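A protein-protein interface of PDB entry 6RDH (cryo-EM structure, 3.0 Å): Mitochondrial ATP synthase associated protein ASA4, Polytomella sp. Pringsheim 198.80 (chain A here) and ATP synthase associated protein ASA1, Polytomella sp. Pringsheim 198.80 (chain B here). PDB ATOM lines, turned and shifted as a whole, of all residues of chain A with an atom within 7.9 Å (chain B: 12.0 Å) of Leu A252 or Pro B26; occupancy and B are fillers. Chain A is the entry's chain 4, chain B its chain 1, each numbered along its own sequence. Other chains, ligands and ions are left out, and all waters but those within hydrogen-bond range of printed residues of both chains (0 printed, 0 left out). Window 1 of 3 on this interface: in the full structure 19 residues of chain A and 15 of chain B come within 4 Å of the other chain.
Of the 8 printed residues of chain B, 5 touch a printed residue of chain A. Printed residues of chain B that touch a printed residue of chain A: Tyr B23, Leu B24, Ala B25, Pro B26 and Leu B27. Hydrophobic or aromatic side chains of chain A within 4 Å of the printed part of chain B: Tyr A249, Leu A252, Trp A264, Tyr A268 and Val A272.
Leu A252 touches just these residues of chain B: Leu B24 and Pro B26. Pro B26 touches just these residues of chain A: Leu A252 (3.7 Å) and Arg A255 (3.8 Å). No residue of chain B comes within 4 Å of Ala A248. No residue of chain B comes within 4 Å of Ser A251. Of the printed residues of chain B, Arg A255 touches Pro B26 (3.8 Å). No residue of chain B comes within 4 Å of Ala A256. Ala B25 touches one residue of chain A. Of the printed residues of chain B, Tyr A268 touches Leu B24 (3.6 Å), Ala B25 (2.8 Å) and Leu B27 (3.5 Å). Of the printed residues of chain A, Tyr B23 touches Tyr A249 and Val A272. Printed residues of chain B within 4 Å of Tyr A249: Tyr B23 (2.9 Å) and Leu B24 (3.6 Å). Of the printed residues of chain A, Leu B27 touches Trp A264 and Tyr A268.
CD2 of Leu B24 touches CE1 of Tyr A249 (3.6 Å). CD1 of Leu A252 touches O of Leu B24 (3.4 Å). CA of Pro B26 touches CD2 of Leu A252, 3.7 Å away. Pro B26 touches Arg A255 (CB to NH2, 3.8 Å). Leu B27 touches Trp A264 (CD2 to CE3, 3.8 Å). Leu B24 touches Tyr A268. CE1 of Tyr A268 touches CD1 of Leu B27, 3.5 Å away. CG1 of Val A272 touches OH of Tyr B23, 3.4 Å away. CG2 of Val A272 touches CD2 of Leu B24 (3.7 Å).
The backbone carbonyl oxygen of Ala B25 lies within hydrogen-bond range of the side-chain hydroxyl of Tyr A268, 2.8 Å away. OH of Tyr B23 lies within hydrogen-bond range of OH of Tyr A249, 2.9 Å away.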
ATOM      1  N   GLN A 245     -21.541  29.720 -12.801  1.00  0.00           N
ATOM      2  CA  GLN A 245     -21.679  28.675 -11.800  1.00  0.00           C
ATOM      3  C   GLN A 245     -22.969  27.892 -11.967  1.00  0.00           C
ATOM      4  O   GLN A 245     -22.985  26.681 -11.725  1.00  0.00           O
ATOM      5  CB  GLN A 245     -21.606  29.281 -10.409  1.00  0.00           C
ATOM      6  CG  GLN A 245     -20.241  29.781 -10.048  1.00  0.00           C
ATOM      7  CD  GLN A 245     -20.098  29.974  -8.575  1.00  0.00           C
ATOM      8  OE1 GLN A 245     -21.086  29.993  -7.850  1.00  0.00           O
ATOM      9  NE2 GLN A 245     -18.868  30.100  -8.110  1.00  0.00           N
ATOM     10  N   ALA A 246     -24.050  28.545 -12.402  1.00  0.00           N
ATOM     11  CA  ALA A 246     -25.288  27.820 -12.648  1.00  0.00           C
ATOM     12  C   ALA A 246     -25.158  26.899 -13.849  1.00  0.00           C
ATOM     13  O   ALA A 246     -25.689  25.784 -13.838  1.00  0.00           O
ATOM     14  CB  ALA A 246     -26.437  28.801 -12.845  1.00  0.00           C
ATOM     15  N   SER A 247     -24.420  27.328 -14.878  1.00  0.00           N
ATOM     16  CA  SER A 247     -24.197  26.476 -16.040  1.00  0.00           C
ATOM     17  C   SER A 247     -23.308  25.291 -15.697  1.00  0.00           C
ATOM     18  O   SER A 247     -23.555  24.174 -16.165  1.00  0.00           O
ATOM     19  CB  SER A 247     -23.582  27.291 -17.169  1.00  0.00           C
ATOM     20  OG  SER A 247     -24.441  28.352 -17.541  1.00  0.00           O
ATOM     21  N   ALA A 248     -22.286  25.508 -14.861  1.00  0.00           N
ATOM     22  CA  ALA A 248     -21.421  24.407 -14.448  1.00  0.00           C
ATOM     23  C   ALA A 248     -22.166  23.405 -13.575  1.00  0.00           C
ATOM     24  O   ALA A 248     -22.014  22.190 -13.755  1.00  0.00           O
ATOM     25  CB  ALA A 248     -20.198  24.946 -13.715  1.00  0.00           C
ATOM     26  N   TYR A 249     -22.992  23.898 -12.646  1.00  0.00           N
ATOM     27  CA  TYR A 249     -23.810  23.021 -11.817  1.00  0.00           C
ATOM     28  C   TYR A 249     -24.799  22.231 -12.655  1.00  0.00           C
ATOM     29  O   TYR A 249     -24.970  21.027 -12.444  1.00  0.00           O
ATOM     30  CB  TYR A 249     -24.554  23.842 -10.768  1.00  0.00           C
ATOM     31  CG  TYR A 249     -25.411  23.036  -9.822  1.00  0.00           C
ATOM     32  CD1 TYR A 249     -24.873  22.487  -8.678  1.00  0.00           C
ATOM     33  CD2 TYR A 249     -26.765  22.848 -10.062  1.00  0.00           C
ATOM     34  CE1 TYR A 249     -25.650  21.763  -7.812  1.00  0.00           C
ATOM     35  CE2 TYR A 249     -27.542  22.116  -9.207  1.00  0.00           C
ATOM     36  CZ  TYR A 249     -26.980  21.579  -8.085  1.00  0.00           C
ATOM     37  OH  TYR A 249     -27.762  20.855  -7.224  1.00  0.00           O
ATOM     38  N   ALA A 250     -25.458  22.890 -13.608  1.00  0.00           N
ATOM     39  CA  ALA A 250     -26.473  22.215 -14.403  1.00  0.00           C
ATOM     40  C   ALA A 250     -25.856  21.192 -15.343  1.00  0.00           C
ATOM     41  O   ALA A 250     -26.431  20.122 -15.559  1.00  0.00           O
ATOM     42  CB  ALA A 250     -27.284  23.244 -15.180  1.00  0.00           C
ATOM     43  N   SER A 251     -24.663  21.476 -15.875  1.00  0.00           N
ATOM     44  CA  SER A 251     -24.009  20.516 -16.757  1.00  0.00           C
ATOM     45  C   SER A 251     -23.489  19.313 -15.983  1.00  0.00           C
ATOM     46  O   SER A 251     -23.651  18.170 -16.427  1.00  0.00           O
ATOM     47  CB  SER A 251     -22.875  21.190 -17.518  1.00  0.00           C
ATOM     48  OG  SER A 251     -21.826  21.552 -16.644  1.00  0.00           O
ATOM     49  N   LEU A 252     -22.879  19.539 -14.816  1.00  0.00           N
ATOM     50  CA  LEU A 252     -22.420  18.417 -14.010  1.00  0.00           C
ATOM     51  C   LEU A 252     -23.562  17.624 -13.394  1.00  0.00           C
ATOM     52  O   LEU A 252     -23.381  16.443 -13.089  1.00  0.00           O
ATOM     53  CB  LEU A 252     -21.505  18.906 -12.903  1.00  0.00           C
ATOM     54  CG  LEU A 252     -20.066  19.277 -13.191  1.00  0.00           C
ATOM     55  CD1 LEU A 252     -19.526  20.102 -12.054  1.00  0.00           C
ATOM     56  CD2 LEU A 252     -19.293  18.007 -13.313  1.00  0.00           C
ATOM     57  N   LEU A 253     -24.726  18.236 -13.197  1.00  0.00           N
ATOM     58  CA  LEU A 253     -25.883  17.482 -12.736  1.00  0.00           C
ATOM     59  C   LEU A 253     -26.533  16.702 -13.865  1.00  0.00           C
ATOM     60  O   LEU A 253     -27.017  15.585 -13.645  1.00  0.00           O
ATOM     61  CB  LEU A 253     -26.896  18.428 -12.108  1.00  0.00           C
ATOM     62  CG  LEU A 253     -27.952  17.793 -11.225  1.00  0.00           C
ATOM     63  CD1 LEU A 253     -27.288  17.092 -10.068  1.00  0.00           C
ATOM     64  CD2 LEU A 253     -28.893  18.864 -10.733  1.00  0.00           C
ATOM     65  N   LYS A 254     -26.550  17.263 -15.077  1.00  0.00           N
ATOM     66  CA  LYS A 254     -27.070  16.530 -16.221  1.00  0.00           C
ATOM     67  C   LYS A 254     -26.164  15.373 -16.599  1.00  0.00           C
ATOM     68  O   LYS A 254     -26.641  14.372 -17.139  1.00  0.00           O
ATOM     69  CB  LYS A 254     -27.248  17.468 -17.409  1.00  0.00           C
ATOM     70  CG  LYS A 254     -28.238  16.962 -18.438  1.00  0.00           C
ATOM     71  CD  LYS A 254     -28.504  17.997 -19.511  1.00  0.00           C
ATOM     72  CE  LYS A 254     -29.581  17.517 -20.465  1.00  0.00           C
ATOM     73  NZ  LYS A 254     -29.240  16.200 -21.068  1.00  0.00           N
ATOM     74  N   ARG A 255     -24.863  15.487 -16.322  1.00  0.00           N
ATOM     75  CA  ARG A 255     -23.958  14.372 -16.574  1.00  0.00           C
ATOM     76  C   ARG A 255     -24.237  13.197 -15.644  1.00  0.00           C
ATOM     77  O   ARG A 255     -24.021  12.043 -16.025  1.00  0.00           O
ATOM     78  CB  ARG A 255     -22.508  14.832 -16.432  1.00  0.00           C
ATOM     79  CG  ARG A 255     -21.488  13.888 -17.035  1.00  0.00           C
ATOM     80  CD  ARG A 255     -20.106  14.151 -16.476  1.00  0.00           C
ATOM     81  NE  ARG A 255     -19.671  15.523 -16.714  1.00  0.00           N
ATOM     82  CZ  ARG A 255     -18.548  16.041 -16.228  1.00  0.00           C
ATOM     83  NH1 ARG A 255     -18.223  17.299 -16.494  1.00  0.00           N
ATOM     84  NH2 ARG A 255     -17.751  15.300 -15.474  1.00  0.00           N
ATOM     85  N   ALA A 256     -24.723  13.462 -14.435  1.00  0.00           N
ATOM     86  CA  ALA A 256     -25.079  12.385 -13.523  1.00  0.00           C
ATOM     87  C   ALA A 256     -26.492  11.876 -13.737  1.00  0.00           C
ATOM     88  O   ALA A 256     -26.780  10.719 -13.420  1.00  0.00           O
ATOM     89  CB  ALA A 256     -24.928  12.839 -12.075  1.00  0.00           C
ATOM     90  N   GLU A 257     -27.388  12.715 -14.242  1.00  0.00           N
ATOM     91  CA  GLU A 257     -28.719  12.228 -14.576  1.00  0.00           C
ATOM     92  C   GLU A 257     -28.781  11.586 -15.954  1.00  0.00           C
ATOM     93  O   GLU A 257     -29.785  10.945 -16.275  1.00  0.00           O
ATOM     94  CB  GLU A 257     -29.724  13.369 -14.478  1.00  0.00           C
ATOM     95  CG  GLU A 257     -29.999  13.772 -13.050  1.00  0.00           C
ATOM     96  CD  GLU A 257     -30.748  15.072 -12.947  1.00  0.00           C
ATOM     97  OE1 GLU A 257     -30.862  15.767 -13.974  1.00  0.00           O
ATOM     98  OE2 GLU A 257     -31.212  15.406 -11.838  1.00  0.00           O
ATOM     99  N   THR A 258     -27.733  11.737 -16.763  1.00  0.00           N
ATOM    100  CA  THR A 258     -27.677  11.063 -18.053  1.00  0.00           C
ATOM    101  C   THR A 258     -27.420   9.575 -17.879  1.00  0.00           C
ATOM    102  O   THR A 258     -28.197   8.739 -18.353  1.00  0.00           O
ATOM    103  CB  THR A 258     -26.591  11.692 -18.919  1.00  0.00           C
ATOM    104  OG1 THR A 258     -26.935  13.053 -19.197  1.00  0.00           O
ATOM    105  CG2 THR A 258     -26.437  10.927 -20.225  1.00  0.00           C
ATOM    106  N   TRP A 264     -22.357   5.049  -9.163  1.00  0.00           N
ATOM    107  CA  TRP A 264     -21.755   6.330  -8.823  1.00  0.00           C
ATOM    108  C   TRP A 264     -22.706   7.480  -9.081  1.00  0.00           C
ATOM    109  O   TRP A 264     -22.696   8.461  -8.337  1.00  0.00           O
ATOM    110  CB  TRP A 264     -20.456   6.531  -9.597  1.00  0.00           C
ATOM    111  CG  TRP A 264     -20.610   6.782 -11.048  1.00  0.00           C
ATOM    112  CD1 TRP A 264     -20.654   5.853 -12.034  1.00  0.00           C
ATOM    113  CD2 TRP A 264     -20.720   8.053 -11.685  1.00  0.00           C
ATOM    114  NE1 TRP A 264     -20.796   6.463 -13.250  1.00  0.00           N
ATOM    115  CE2 TRP A 264     -20.841   7.818 -13.061  1.00  0.00           C
ATOM    116  CE3 TRP A 264     -20.740   9.368 -11.222  1.00  0.00           C
ATOM    117  CZ2 TRP A 264     -20.974   8.848 -13.980  1.00  0.00           C
ATOM    118  CZ3 TRP A 264     -20.872  10.387 -12.134  1.00  0.00           C
ATOM    119  CH2 TRP A 264     -20.987  10.123 -13.498  1.00  0.00           C
ATOM    120  N   TYR A 268     -24.109   9.995  -6.385  1.00  0.00           N
ATOM    121  CA  TYR A 268     -23.958  11.420  -6.663  1.00  0.00           C
ATOM    122  C   TYR A 268     -25.254  12.177  -6.402  1.00  0.00           C
ATOM    123  O   TYR A 268     -25.258  13.234  -5.760  1.00  0.00           O
ATOM    124  CB  TYR A 268     -23.530  11.587  -8.118  1.00  0.00           C
ATOM    125  CG  TYR A 268     -22.805  12.855  -8.478  1.00  0.00           C
ATOM    126  CD1 TYR A 268     -21.437  12.945  -8.358  1.00  0.00           C
ATOM    127  CD2 TYR A 268     -23.491  13.945  -8.983  1.00  0.00           C
ATOM    128  CE1 TYR A 268     -20.773  14.093  -8.705  1.00  0.00           C
ATOM    129  CE2 TYR A 268     -22.826  15.098  -9.335  1.00  0.00           C
ATOM    130  CZ  TYR A 268     -21.467  15.158  -9.192  1.00  0.00           C
ATOM    131  OH  TYR A 268     -20.774  16.288  -9.529  1.00  0.00           O
ATOM    132  N   LEU A 269     -26.374  11.638  -6.878  1.00  0.00           N
ATOM    133  CA  LEU A 269     -27.644  12.323  -6.678  1.00  0.00           C
ATOM    134  C   LEU A 269     -28.125  12.220  -5.235  1.00  0.00           C
ATOM    135  O   LEU A 269     -28.761  13.155  -4.731  1.00  0.00           O
ATOM    136  CB  LEU A 269     -28.683  11.775  -7.647  1.00  0.00           C
ATOM    137  CG  LEU A 269     -28.330  11.981  -9.119  1.00  0.00           C
ATOM    138  CD1 LEU A 269     -29.484  11.567 -10.000  1.00  0.00           C
ATOM    139  CD2 LEU A 269     -27.937  13.420  -9.395  1.00  0.00           C
ATOM    140  N   VAL A 272     -26.277  14.993  -3.587  1.00  0.00           N
ATOM    141  CA  VAL A 272     -26.917  16.281  -3.856  1.00  0.00           C
ATOM    142  C   VAL A 272     -28.137  16.469  -2.959  1.00  0.00           C
ATOM    143  O   VAL A 272     -28.351  17.550  -2.388  1.00  0.00           O
ATOM    144  CB  VAL A 272     -27.282  16.383  -5.346  1.00  0.00           C
ATOM    145  CG1 VAL A 272     -28.091  17.621  -5.620  1.00  0.00           C
ATOM    146  CG2 VAL A 272     -26.038  16.398  -6.161  1.00  0.00           C
ATOM    147  N   TYR B  23     -21.762  23.528  -6.321  1.00  0.00           N
ATOM    148  CA  TYR B  23     -20.942  23.132  -5.189  1.00  0.00           C
ATOM    149  C   TYR B  23     -20.287  21.804  -5.462  1.00  0.00           C
ATOM    150  O   TYR B  23     -19.414  21.364  -4.727  1.00  0.00           O
ATOM    151  CB  TYR B  23     -21.774  23.044  -3.917  1.00  0.00           C
ATOM    152  CG  TYR B  23     -23.118  22.382  -4.079  1.00  0.00           C
ATOM    153  CD1 TYR B  23     -24.258  23.143  -4.249  1.00  0.00           C
ATOM    154  CD2 TYR B  23     -23.251  21.003  -4.032  1.00  0.00           C
ATOM    155  CE1 TYR B  23     -25.484  22.555  -4.388  1.00  0.00           C
ATOM    156  CE2 TYR B  23     -24.477  20.407  -4.172  1.00  0.00           C
ATOM    157  CZ  TYR B  23     -25.588  21.190  -4.352  1.00  0.00           C
ATOM    158  OH  TYR B  23     -26.826  20.620  -4.492  1.00  0.00           O
ATOM    159  N   LEU B  24     -20.726  21.158  -6.526  1.00  0.00           N
ATOM    160  CA  LEU B  24     -20.266  19.826  -6.871  1.00  0.00           C
ATOM    161  C   LEU B  24     -19.187  19.868  -7.943  1.00  0.00           C
ATOM    162  O   LEU B  24     -19.132  20.783  -8.766  1.00  0.00           O
ATOM    163  CB  LEU B  24     -21.452  18.958  -7.289  1.00  0.00           C
ATOM    164  CG  LEU B  24     -22.597  19.579  -8.075  1.00  0.00           C
ATOM    165  CD1 LEU B  24     -22.290  19.704  -9.498  1.00  0.00           C
ATOM    166  CD2 LEU B  24     -23.782  18.702  -7.915  1.00  0.00           C
ATOM    167  N   ALA B  25     -18.321  18.866  -7.906  1.00  0.00           N
ATOM    168  CA  ALA B  25     -17.106  18.790  -8.692  1.00  0.00           C
ATOM    169  C   ALA B  25     -17.181  17.616  -9.654  1.00  0.00           C
ATOM    170  O   ALA B  25     -17.960  16.680  -9.439  1.00  0.00           O
ATOM    171  CB  ALA B  25     -15.892  18.631  -7.767  1.00  0.00           C
ATOM    172  N   PRO B  26     -16.412  17.640 -10.744  1.00  0.00           N
ATOM    173  CA  PRO B  26     -16.357  16.465 -11.621  1.00  0.00           C
ATOM    174  C   PRO B  26     -15.613  15.312 -10.968  1.00  0.00           C
ATOM    175  O   PRO B  26     -14.493  15.468 -10.484  1.00  0.00           O
ATOM    176  CB  PRO B  26     -15.617  16.979 -12.859  1.00  0.00           C
ATOM    177  CG  PRO B  26     -14.937  18.206 -12.417  1.00  0.00           C
ATOM    178  CD  PRO B  26     -15.821  18.817 -11.396  1.00  0.00           C
ATOM    179  N   LEU B  27     -16.255  14.153 -10.955  1.00  0.00           N
ATOM    180  CA  LEU B  27     -15.644  12.933 -10.453  1.00  0.00           C
ATOM    181  C   LEU B  27     -14.607  12.407 -11.435  1.00  0.00           C
ATOM    182  O   LEU B  27     -14.914  12.158 -12.604  1.00  0.00           O
ATOM    183  CB  LEU B  27     -16.721  11.891 -10.175  1.00  0.00           C
ATOM    184  CG  LEU B  27     -17.099  11.680  -8.712  1.00  0.00           C
ATOM    185  CD1 LEU B  27     -17.511  12.948  -8.040  1.00  0.00           C
ATOM    186  CD2 LEU B  27     -18.223  10.674  -8.633  1.00  0.00           C
ATOM    187  N   ARG B  28     -13.378  12.246 -10.954  1.00  0.00           N
ATOM    188  CA  ARG B  28     -12.274  11.707 -11.725  1.00  0.00           C
ATOM    189  C   ARG B  28     -11.810  10.399 -11.105  1.00  0.00           C
ATOM    190  O   ARG B  28     -11.887  10.210  -9.890  1.00  0.00           O
ATOM    191  CB  ARG B  28     -11.112  12.687 -11.769  1.00  0.00           C
ATOM    192  CG  ARG B  28     -11.477  14.035 -12.325  1.00  0.00           C
ATOM    193  CD  ARG B  28     -10.340  15.002 -12.159  1.00  0.00           C
ATOM    194  NE  ARG B  28      -9.073  14.370 -12.483  1.00  0.00           N
ATOM    195  CZ  ARG B  28      -7.913  15.005 -12.478  1.00  0.00           C
ATOM    196  NH1 ARG B  28      -6.802  14.357 -12.781  1.00  0.00           N
ATOM    197  NH2 ARG B  28      -7.876  16.293 -12.178  1.00  0.00           N
ATOM    198  N   SER B  29     -11.357   9.479 -11.951  1.00  0.00           N
ATOM    199  CA  SER B  29     -10.757   8.233 -11.490  1.00  0.00           C
ATOM    200  C   SER B  29      -9.467   8.043 -12.275  1.00  0.00           C
ATOM    201  O   SER B  29      -9.423   7.311 -13.262  1.00  0.00           O
ATOM    202  CB  SER B  29     -11.700   7.059 -11.689  1.00  0.00           C
ATOM    203  OG  SER B  29     -11.910   6.818 -13.070  1.00  0.00           O
ATOM    204  N   ASP B  30      -8.400   8.683 -11.815  1.00  0.00           N
ATOM    205  CA  ASP B  30      -7.106   8.529 -12.450  1.00  0.00           C
ATOM    206  C   ASP B  30      -6.035   8.703 -11.392  1.00  0.00           C
ATOM    207  O   ASP B  30      -6.260   9.316 -10.348  1.00  0.00           O
ATOM    208  CB  ASP B  30      -6.903   9.512 -13.607  1.00  0.00           C
ATOM    209  CG  ASP B  30      -6.960  10.954 -13.168  1.00  0.00           C
ATOM    210  OD1 ASP B  30      -7.694  11.249 -12.213  1.00  0.00           O
ATOM    211  OD2 ASP B  30      -6.275  11.798 -13.778  1.00  0.00           O
